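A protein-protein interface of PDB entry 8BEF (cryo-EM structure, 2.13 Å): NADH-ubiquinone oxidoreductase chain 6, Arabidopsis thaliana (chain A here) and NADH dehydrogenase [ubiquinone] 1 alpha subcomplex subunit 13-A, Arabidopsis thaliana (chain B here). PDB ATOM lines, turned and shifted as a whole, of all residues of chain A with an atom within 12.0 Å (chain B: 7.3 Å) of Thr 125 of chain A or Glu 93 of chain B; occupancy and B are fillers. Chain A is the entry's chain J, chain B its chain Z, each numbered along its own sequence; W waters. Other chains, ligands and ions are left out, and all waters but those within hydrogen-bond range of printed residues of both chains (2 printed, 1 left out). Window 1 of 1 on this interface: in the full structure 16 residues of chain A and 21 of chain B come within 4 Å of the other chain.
Printed residues of chain B that touch a printed residue of chain A: Leu 89, Gln 90, Glu 93, Asp 94, Arg 96, Phe 97 and Asp 141. Hydrophobic or aromatic side chains of chain B within 4 Å of the printed part of chain A: Leu 89 and Phe 97. Of the 13 printed residues of chain A, 8 touch a printed residue of chain B. Hydrophobic or aromatic side chains of chain A that line the printed part of chain B: Tyr 124 and Tyr 127. Among the printed residues, 15 pairs touch across the chains. Among the printed residues, Asp or Glu carboxylates within 4 Å of a Lys or Arg side-chain nitrogen of the other chain: Lys 130 of chain A with Asp 141 of chain B (3.3 Å).
Water W2 lies within hydrogen-bond range of the side-chain hydroxyl of Tyr 127 of chain A (2.6 Å), the side-chain carboxylate of Glu 92 of chain B (3.1 Å) and the backbone carbonyl oxygen of Leu 89 of chain B (3.2 Å). Water W1 lies within hydrogen-bond range of the side-chain amide oxygen (OE1) of Gln 90 of chain B (2.7 Å), the backbone NH (N) of Ala 128 of chain A (2.8 Å) and the backbone NH (N) of Tyr 127 of chain A (3.2 Å).
OE2 of Glu 93 of chain B lies within hydrogen-bond range of N of Thr 125 of chain A (2.9 Å). The side-chain amide oxygen of Gln 90 of chain B sits at hydrogen-bond distance from the backbone NH of Tyr 127 of chain A. The guanidinium group (NH2) of Arg 96 of chain B is in hydrogen-bond range of the backbone carbonyl oxygen (O) of Arg 123 of chain A (3.2 Å). NE2 of Gln 90 of chain B is in hydrogen-bond range of OH of Tyr 124 of chain A, at 3.1 Å. The side-chain carboxylate of Asp 141 of chain B lies within salt-bridge range of the side-chain amino group of Lys 130 of chain A, at 3.3 Å. The side-chain amide nitrogen (NE2) of Gln 90 of chain B lies within hydrogen-bond range of the backbone carbonyl oxygen (O) of Thr 125 of chain A (3.2 Å). OD1 of Asp 94 of chain B lies within hydrogen-bond range of OH of Tyr 124 of chain A (2.4 Å). The backbone carbonyl oxygen of Ser 121 of chain A is in hydrogen-bond range of the guanidinium group of Arg 96 of chain B.
The side-chain amide nitrogen (NE2) of Gln 90 of chain B lies within hydrogen-bond range of the side-chain carboxylate (OD1) of Asp 94 of chain B (3.2 Å). NH2 of Arg 96 of chain B is in salt-bridge range of OE2 of Glu 93 of chain B. The side-chain hydroxyl (OG) of Ser 99 of chain B is in hydrogen-bond range of the backbone carbonyl oxygen (O) of Arg 96 of chain B (2.7 Å).
Printed residues of chain B within 4 Å of Arg 123 of chain A: Glu 93 (3.6 Å) and Arg 96 (3.2 Å). Of the printed residues of chain B, Tyr 124 of chain A touches Gln 90, Glu 93, Asp 94 and Phe 97. Thr 125 of chain A touches two residues of chain B. Ile 88 of chain B touches none of the printed residues of chain A. Of the printed residues of chain A, Leu 89 of chain B touches Tyr 127. No residue of chain A comes within 4 Å of Ala 91 of chain B. Glu 92 of chain B touches none of the printed residues of chain A. Glu 93 of chain B touches four residues of chain A. Asp 94 of chain B touches one residue of chain A. Of chain A, only Leu 122 and Tyr 124 come within 4 Å of Phe 97 of chain B. Ser 99 of chain B touches none of the printed residues of chain A. Of the printed residues of chain A, Asp 141 of chain B touches Lys 130 (3.3 Å).
O of Leu 122 of chain A touches CE1 of Phe 97 of chain B, at 3.3 Å. Arg 123 of chain A touches Glu 93 of chain B. OE2 of Glu 93 of chain B touches CA of Tyr 124 of chain A (3.6 Å). Phe 97 of chain B touches Tyr 124 of chain A (CB to CD1, 3.98 Å). CA of Val 126 of chain A touches OE1 of Gln 90 of chain B (3.6 Å). Tyr 127 of chain A touches Leu 89 of chain B (CE2 to O, 3.5 Å). Glu 93 of chain B touches Tyr 127 of chain A (CB to CE2, 3.9 Å).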
ATOM      1  N   THR A 119      16.553 -28.825  16.962  1.00  0.00           N
ATOM      2  CA  THR A 119      15.797 -27.583  17.027  1.00  0.00           C
ATOM      3  C   THR A 119      15.091 -27.402  18.365  1.00  0.00           C
ATOM      4  O   THR A 119      14.582 -26.309  18.638  1.00  0.00           O
ATOM      5  CB  THR A 119      14.773 -27.532  15.888  1.00  0.00           C
ATOM      6  OG1 THR A 119      15.329 -28.147  14.719  1.00  0.00           O
ATOM      7  CG2 THR A 119      14.408 -26.092  15.551  1.00  0.00           C
ATOM      8  N   THR A 120      15.065 -28.438  19.209  1.00  0.00           N
ATOM      9  CA  THR A 120      14.364 -28.345  20.487  1.00  0.00           C
ATOM     10  C   THR A 120      14.930 -27.240  21.369  1.00  0.00           C
ATOM     11  O   THR A 120      14.204 -26.671  22.191  1.00  0.00           O
ATOM     12  CB  THR A 120      14.425 -29.684  21.221  1.00  0.00           C
ATOM     13  OG1 THR A 120      15.783 -29.979  21.573  1.00  0.00           O
ATOM     14  CG2 THR A 120      13.878 -30.801  20.344  1.00  0.00           C
ATOM     15  N   SER A 121      16.212 -26.910  21.206  1.00  0.00           N
ATOM     16  CA  SER A 121      16.808 -25.854  22.014  1.00  0.00           C
ATOM     17  C   SER A 121      16.291 -24.473  21.635  1.00  0.00           C
ATOM     18  O   SER A 121      16.437 -23.535  22.424  1.00  0.00           O
ATOM     19  CB  SER A 121      18.328 -25.890  21.888  1.00  0.00           C
ATOM     20  OG  SER A 121      18.769 -25.011  20.871  1.00  0.00           O
ATOM     21  N   LEU A 122      15.695 -24.325  20.457  1.00  0.00           N
ATOM     22  CA  LEU A 122      15.140 -23.050  20.028  1.00  0.00           C
ATOM     23  C   LEU A 122      13.706 -22.840  20.490  1.00  0.00           C
ATOM     24  O   LEU A 122      13.109 -21.812  20.159  1.00  0.00           O
ATOM     25  CB  LEU A 122      15.225 -22.921  18.504  1.00  0.00           C
ATOM     26  CG  LEU A 122      16.645 -22.727  17.965  1.00  0.00           C
ATOM     27  CD1 LEU A 122      16.620 -22.154  16.562  1.00  0.00           C
ATOM     28  CD2 LEU A 122      17.439 -21.822  18.889  1.00  0.00           C
ATOM     29  N   ARG A 123      13.141 -23.785  21.237  1.00  0.00           N
ATOM     30  CA  ARG A 123      11.837 -23.578  21.850  1.00  0.00           C
ATOM     31  C   ARG A 123      11.960 -22.535  22.955  1.00  0.00           C
ATOM     32  O   ARG A 123      12.710 -22.725  23.917  1.00  0.00           O
ATOM     33  CB  ARG A 123      11.296 -24.895  22.404  1.00  0.00           C
ATOM     34  CG  ARG A 123       9.831 -25.150  22.083  1.00  0.00           C
ATOM     35  CD  ARG A 123       9.533 -26.636  21.940  1.00  0.00           C
ATOM     36  NE  ARG A 123      10.014 -27.176  20.674  1.00  0.00           N
ATOM     37  CZ  ARG A 123       9.974 -28.460  20.343  1.00  0.00           C
ATOM     38  NH1 ARG A 123       9.475 -29.370  21.163  1.00  0.00           N
ATOM     39  NH2 ARG A 123      10.445 -28.840  19.158  1.00  0.00           N
ATOM     40  N   TYR A 124      11.235 -21.430  22.813  1.00  0.00           N
ATOM     41  CA  TYR A 124      11.257 -20.354  23.795  1.00  0.00           C
ATOM     42  C   TYR A 124      10.121 -20.550  24.792  1.00  0.00           C
ATOM     43  O   TYR A 124       8.969 -20.744  24.397  1.00  0.00           O
ATOM     44  CB  TYR A 124      11.132 -18.996  23.102  1.00  0.00           C
ATOM     45  CG  TYR A 124      11.211 -17.810  24.037  1.00  0.00           C
ATOM     46  CD1 TYR A 124      12.257 -17.683  24.943  1.00  0.00           C
ATOM     47  CD2 TYR A 124      10.240 -16.819  24.015  1.00  0.00           C
ATOM     48  CE1 TYR A 124      12.334 -16.607  25.795  1.00  0.00           C
ATOM     49  CE2 TYR A 124      10.307 -15.738  24.868  1.00  0.00           C
ATOM     50  CZ  TYR A 124      11.356 -15.637  25.756  1.00  0.00           C
ATOM     51  OH  TYR A 124      11.425 -14.563  26.605  1.00  0.00           O
ATOM     52  N   THR A 125      10.448 -20.492  26.080  1.00  0.00           N
ATOM     53  CA  THR A 125       9.481 -20.708  27.151  1.00  0.00           C
ATOM     54  C   THR A 125       9.121 -19.374  27.792  1.00  0.00           C
ATOM     55  O   THR A 125      10.005 -18.639  28.243  1.00  0.00           O
ATOM     56  CB  THR A 125      10.034 -21.668  28.203  1.00  0.00           C
ATOM     57  OG1 THR A 125      10.147 -22.980  27.638  1.00  0.00           O
ATOM     58  CG2 THR A 125       9.125 -21.717  29.416  1.00  0.00           C
ATOM     59  N   VAL A 126       7.829 -19.072  27.835  1.00  0.00           N
ATOM     60  CA  VAL A 126       7.300 -17.907  28.536  1.00  0.00           C
ATOM     61  C   VAL A 126       6.609 -18.417  29.791  1.00  0.00           C
ATOM     62  O   VAL A 126       5.542 -19.037  29.714  1.00  0.00           O
ATOM     63  CB  VAL A 126       6.333 -17.100  27.659  1.00  0.00           C
ATOM     64  CG1 VAL A 126       5.874 -15.842  28.391  1.00  0.00           C
ATOM     65  CG2 VAL A 126       6.980 -16.757  26.331  1.00  0.00           C
ATOM     66  N   TYR A 127       7.212 -18.161  30.954  1.00  0.00           N
ATOM     67  CA  TYR A 127       6.640 -18.666  32.194  1.00  0.00           C
ATOM     68  C   TYR A 127       5.413 -17.875  32.634  1.00  0.00           C
ATOM     69  O   TYR A 127       4.663 -18.353  33.490  1.00  0.00           O
ATOM     70  CB  TYR A 127       7.685 -18.653  33.313  1.00  0.00           C
ATOM     71  CG  TYR A 127       8.868 -19.574  33.118  1.00  0.00           C
ATOM     72  CD1 TYR A 127       8.787 -20.916  33.451  1.00  0.00           C
ATOM     73  CD2 TYR A 127      10.080 -19.090  32.636  1.00  0.00           C
ATOM     74  CE1 TYR A 127       9.865 -21.760  33.285  1.00  0.00           C
ATOM     75  CE2 TYR A 127      11.166 -19.925  32.469  1.00  0.00           C
ATOM     76  CZ  TYR A 127      11.052 -21.263  32.798  1.00  0.00           C
ATOM     77  OH  TYR A 127      12.121 -22.111  32.638  1.00  0.00           O
ATOM     78  N   ALA A 128       5.189 -16.687  32.064  1.00  0.00           N
ATOM     79  CA  ALA A 128       4.085 -15.844  32.515  1.00  0.00           C
ATOM     80  C   ALA A 128       2.740 -16.531  32.312  1.00  0.00           C
ATOM     81  O   ALA A 128       1.865 -16.470  33.184  1.00  0.00           O
ATOM     82  CB  ALA A 128       4.118 -14.501  31.789  1.00  0.00           C
ATOM     83  N   GLY A 129       2.557 -17.197  31.175  1.00  0.00           N
ATOM     84  CA  GLY A 129       1.323 -17.918  30.928  1.00  0.00           C
ATOM     85  C   GLY A 129       1.175 -19.204  31.715  1.00  0.00           C
ATOM     86  O   GLY A 129       0.112 -19.830  31.641  1.00  0.00           O
ATOM     87  N   LYS A 130       2.198 -19.605  32.466  1.00  0.00           N
ATOM     88  CA  LYS A 130       2.192 -20.860  33.208  1.00  0.00           C
ATOM     89  C   LYS A 130       1.906 -20.689  34.695  1.00  0.00           C
ATOM     90  O   LYS A 130       1.865 -21.688  35.418  1.00  0.00           O
ATOM     91  CB  LYS A 130       3.533 -21.582  33.032  1.00  0.00           C
ATOM     92  CG  LYS A 130       3.690 -22.322  31.721  1.00  0.00           C
ATOM     93  CD  LYS A 130       5.135 -22.722  31.486  1.00  0.00           C
ATOM     94  CE  LYS A 130       5.392 -23.032  30.026  1.00  0.00           C
ATOM     95  NZ  LYS A 130       5.559 -24.488  29.797  1.00  0.00           N
ATOM     96  N   VAL A 131       1.729 -19.455  35.172  1.00  0.00           N
ATOM     97  CA  VAL A 131       1.458 -19.235  36.591  1.00  0.00           C
ATOM     98  C   VAL A 131       0.102 -19.819  36.968  1.00  0.00           C
ATOM     99  O   VAL A 131      -0.039 -20.488  37.995  1.00  0.00           O
ATOM    100  CB  VAL A 131       1.542 -17.731  36.920  1.00  0.00           C
ATOM    101  CG1 VAL A 131       0.933 -17.436  38.283  1.00  0.00           C
ATOM    102  CG2 VAL A 131       2.984 -17.231  36.836  1.00  0.00           C
ATOM    103  N   PRO B  87      10.452 -13.475  37.457  1.00  0.00           N
ATOM    104  CA  PRO B  87      11.467 -12.726  36.692  1.00  0.00           C
ATOM    105  C   PRO B  87      12.808 -13.429  36.556  1.00  0.00           C
ATOM    106  O   PRO B  87      13.397 -13.381  35.473  1.00  0.00           O
ATOM    107  CB  PRO B  87      11.586 -11.412  37.476  1.00  0.00           C
ATOM    108  CG  PRO B  87      10.275 -11.264  38.137  1.00  0.00           C
ATOM    109  CD  PRO B  87       9.878 -12.644  38.532  1.00  0.00           C
ATOM    110  N   ILE B  88      13.308 -14.089  37.602  1.00  0.00           N
ATOM    111  CA  ILE B  88      14.623 -14.718  37.495  1.00  0.00           C
ATOM    112  C   ILE B  88      14.573 -15.926  36.564  1.00  0.00           C
ATOM    113  O   ILE B  88      15.494 -16.153  35.768  1.00  0.00           O
ATOM    114  CB  ILE B  88      15.177 -15.081  38.888  1.00  0.00           C
ATOM    115  CG1 ILE B  88      16.624 -15.560  38.756  1.00  0.00           C
ATOM    116  CG2 ILE B  88      14.306 -16.114  39.597  1.00  0.00           C
ATOM    117  CD1 ILE B  88      17.232 -16.052  40.034  1.00  0.00           C
ATOM    118  N   LEU B  89      13.492 -16.709  36.630  1.00  0.00           N
ATOM    119  CA  LEU B  89      13.336 -17.823  35.701  1.00  0.00           C
ATOM    120  C   LEU B  89      13.261 -17.326  34.262  1.00  0.00           C
ATOM    121  O   LEU B  89      13.893 -17.898  33.363  1.00  0.00           O
ATOM    122  CB  LEU B  89      12.091 -18.632  36.064  1.00  0.00           C
ATOM    123  CG  LEU B  89      12.083 -19.221  37.477  1.00  0.00           C
ATOM    124  CD1 LEU B  89      10.688 -19.687  37.878  1.00  0.00           C
ATOM    125  CD2 LEU B  89      13.087 -20.363  37.592  1.00  0.00           C
ATOM    126  N   GLN B  90      12.508 -16.248  34.031  1.00  0.00           N
ATOM    127  CA  GLN B  90      12.406 -15.697  32.684  1.00  0.00           C
ATOM    128  C   GLN B  90      13.749 -15.163  32.199  1.00  0.00           C
ATOM    129  O   GLN B  90      14.091 -15.321  31.028  1.00  0.00           O
ATOM    130  CB  GLN B  90      11.347 -14.598  32.637  1.00  0.00           C
ATOM    131  CG  GLN B  90      10.740 -14.380  31.261  1.00  0.00           C
ATOM    132  CD  GLN B  90      10.499 -15.674  30.508  1.00  0.00           C
ATOM    133  OE1 GLN B  90       9.625 -16.459  30.869  1.00  0.00           O
ATOM    134  NE2 GLN B  90      11.268 -15.900  29.451  1.00  0.00           N
ATOM    135  N   ALA B  91      14.514 -14.514  33.082  1.00  0.00           N
ATOM    136  CA  ALA B  91      15.819 -13.986  32.690  1.00  0.00           C
ATOM    137  C   ALA B  91      16.780 -15.108  32.320  1.00  0.00           C
ATOM    138  O   ALA B  91      17.514 -15.010  31.326  1.00  0.00           O
ATOM    139  CB  ALA B  91      16.395 -13.137  33.822  1.00  0.00           C
ATOM    140  N   GLU B  92      16.790 -16.182  33.112  1.00  0.00           N
ATOM    141  CA  GLU B  92      17.582 -17.358  32.770  1.00  0.00           C
ATOM    142  C   GLU B  92      17.181 -17.910  31.408  1.00  0.00           C
ATOM    143  O   GLU B  92      18.039 -18.214  30.567  1.00  0.00           O
ATOM    144  CB  GLU B  92      17.407 -18.420  33.851  1.00  0.00           C
ATOM    145  CG  GLU B  92      18.221 -19.672  33.645  1.00  0.00           C
ATOM    146  CD  GLU B  92      17.964 -20.697  34.728  1.00  0.00           C
ATOM    147  OE1 GLU B  92      18.577 -20.587  35.807  1.00  0.00           O
ATOM    148  OE2 GLU B  92      17.150 -21.614  34.498  1.00  0.00           O
ATOM    149  N   GLU B  93      15.873 -18.044  31.171  1.00  0.00           N
ATOM    150  CA  GLU B  93      15.409 -18.566  29.891  1.00  0.00           C
ATOM    151  C   GLU B  93      15.804 -17.645  28.743  1.00  0.00           C
ATOM    152  O   GLU B  93      16.155 -18.113  27.655  1.00  0.00           O
ATOM    153  CB  GLU B  93      13.893 -18.776  29.919  1.00  0.00           C
ATOM    154  CG  GLU B  93      13.275 -19.061  28.555  1.00  0.00           C
ATOM    155  CD  GLU B  93      13.660 -20.417  27.974  1.00  0.00           C
ATOM    156  OE1 GLU B  93      14.439 -21.161  28.606  1.00  0.00           O
ATOM    157  OE2 GLU B  93      13.192 -20.731  26.863  1.00  0.00           O
ATOM    158  N   ASP B  94      15.751 -16.331  28.968  1.00  0.00           N
ATOM    159  CA  ASP B  94      16.126 -15.381  27.926  1.00  0.00           C
ATOM    160  C   ASP B  94      17.599 -15.515  27.568  1.00  0.00           C
ATOM    161  O   ASP B  94      17.963 -15.538  26.387  1.00  0.00           O
ATOM    162  CB  ASP B  94      15.810 -13.955  28.379  1.00  0.00           C
ATOM    163  CG  ASP B  94      14.338 -13.614  28.256  1.00  0.00           C
ATOM    164  OD1 ASP B  94      13.570 -14.455  27.744  1.00  0.00           O
ATOM    165  OD2 ASP B  94      13.954 -12.498  28.660  1.00  0.00           O
ATOM    166  N   GLU B  95      18.465 -15.611  28.579  1.00  0.00           N
ATOM    167  CA  GLU B  95      19.890 -15.795  28.306  1.00  0.00           C
ATOM    168  C   GLU B  95      20.143 -17.096  27.550  1.00  0.00           C
ATOM    169  O   GLU B  95      20.898 -17.122  26.564  1.00  0.00           O
ATOM    170  CB  GLU B  95      20.680 -15.766  29.614  1.00  0.00           C
ATOM    171  CG  GLU B  95      20.908 -14.367  30.166  1.00  0.00           C
ATOM    172  CD  GLU B  95      22.096 -13.673  29.533  1.00  0.00           C
ATOM    173  OE1 GLU B  95      22.611 -14.174  28.512  1.00  0.00           O
ATOM    174  OE2 GLU B  95      22.522 -12.624  30.060  1.00  0.00           O
ATOM    175  N   ARG B  96      19.496 -18.182  27.985  1.00  0.00           N
ATOM    176  CA  ARG B  96      19.639 -19.464  27.300  1.00  0.00           C
ATOM    177  C   ARG B  96      19.223 -19.365  25.837  1.00  0.00           C
ATOM    178  O   ARG B  96      19.947 -19.814  24.938  1.00  0.00           O
ATOM    179  CB  ARG B  96      18.813 -20.530  28.022  1.00  0.00           C
ATOM    180  CG  ARG B  96      19.208 -21.953  27.695  1.00  0.00           C
ATOM    181  CD  ARG B  96      18.022 -22.900  27.826  1.00  0.00           C
ATOM    182  NE  ARG B  96      16.821 -22.385  27.181  1.00  0.00           N
ATOM    183  CZ  ARG B  96      16.531 -22.549  25.897  1.00  0.00           C
ATOM    184  NH1 ARG B  96      17.335 -23.213  25.085  1.00  0.00           N
ATOM    185  NH2 ARG B  96      15.407 -22.028  25.416  1.00  0.00           N
ATOM    186  N   PHE B  97      18.054 -18.770  25.582  1.00  0.00           N
ATOM    187  CA  PHE B  97      17.563 -18.676  24.214  1.00  0.00           C
ATOM    188  C   PHE B  97      18.458 -17.789  23.362  1.00  0.00           C
ATOM    189  O   PHE B  97      18.660 -18.071  22.180  1.00  0.00           O
ATOM    190  CB  PHE B  97      16.132 -18.150  24.179  1.00  0.00           C
ATOM    191  CG  PHE B  97      15.594 -17.999  22.787  1.00  0.00           C
ATOM    192  CD1 PHE B  97      15.044 -19.083  22.125  1.00  0.00           C
ATOM    193  CD2 PHE B  97      15.674 -16.787  22.125  1.00  0.00           C
ATOM    194  CE1 PHE B  97      14.563 -18.953  20.838  1.00  0.00           C
ATOM    195  CE2 PHE B  97      15.201 -16.654  20.837  1.00  0.00           C
ATOM    196  CZ  PHE B  97      14.640 -17.738  20.195  1.00  0.00           C
ATOM    197  N   VAL B  98      18.971 -16.696  23.926  1.00  0.00           N
ATOM    198  CA  VAL B  98      19.823 -15.807  23.143  1.00  0.00           C
ATOM    199  C   VAL B  98      21.108 -16.519  22.740  1.00  0.00           C
ATOM    200  O   VAL B  98      21.546 -16.429  21.587  1.00  0.00           O
ATOM    201  CB  VAL B  98      20.102 -14.506  23.918  1.00  0.00           C
ATOM    202  CG1 VAL B  98      21.232 -13.734  23.267  1.00  0.00           C
ATOM    203  CG2 VAL B  98      18.854 -13.653  23.968  1.00  0.00           C
ATOM    204  N   SER B  99      21.724 -17.248  23.674  1.00  0.00           N
ATOM    205  CA  SER B  99      22.932 -17.996  23.332  1.00  0.00           C
ATOM    206  C   SER B  99      22.646 -19.045  22.258  1.00  0.00           C
ATOM    207  O   SER B  99      23.402 -19.184  21.283  1.00  0.00           O
ATOM    208  CB  SER B  99      23.510 -18.650  24.585  1.00  0.00           C
ATOM    209  OG  SER B  99      22.614 -19.609  25.114  1.00  0.00           O
ATOM    210  N   PRO B 132       8.721 -15.889  18.661  1.00  0.00           N
ATOM    211  CA  PRO B 132       9.537 -17.080  18.870  1.00  0.00           C
ATOM    212  C   PRO B 132       9.542 -17.943  17.626  1.00  0.00           C
ATOM    213  O   PRO B 132       8.587 -17.915  16.826  1.00  0.00           O
ATOM    214  CB  PRO B 132       8.843 -17.789  20.046  1.00  0.00           C
ATOM    215  CG  PRO B 132       7.829 -16.851  20.577  1.00  0.00           C
ATOM    216  CD  PRO B 132       7.538 -15.834  19.535  1.00  0.00           C
ATOM    217  N   ASP B 141       3.255 -28.197  24.136  1.00  0.00           N
ATOM    218  CA  ASP B 141       3.341 -27.788  25.536  1.00  0.00           C
ATOM    219  C   ASP B 141       2.628 -28.736  26.495  1.00  0.00           C
ATOM    220  O   ASP B 141       2.889 -28.678  27.700  1.00  0.00           O
ATOM    221  CB  ASP B 141       2.774 -26.378  25.705  1.00  0.00           C
ATOM    222  CG  ASP B 141       3.350 -25.661  26.910  1.00  0.00           C
ATOM    223  OD1 ASP B 141       2.799 -25.821  28.020  1.00  0.00           O
ATOM    224  OD2 ASP B 141       4.352 -24.935  26.745  1.00  0.00           O
HETATM  225  O   HOH W   1       7.344 -15.015  31.302  1.00  0.00           O
HETATM  226  O   HOH W   2      14.374 -21.093  33.286  1.00  0.00           O
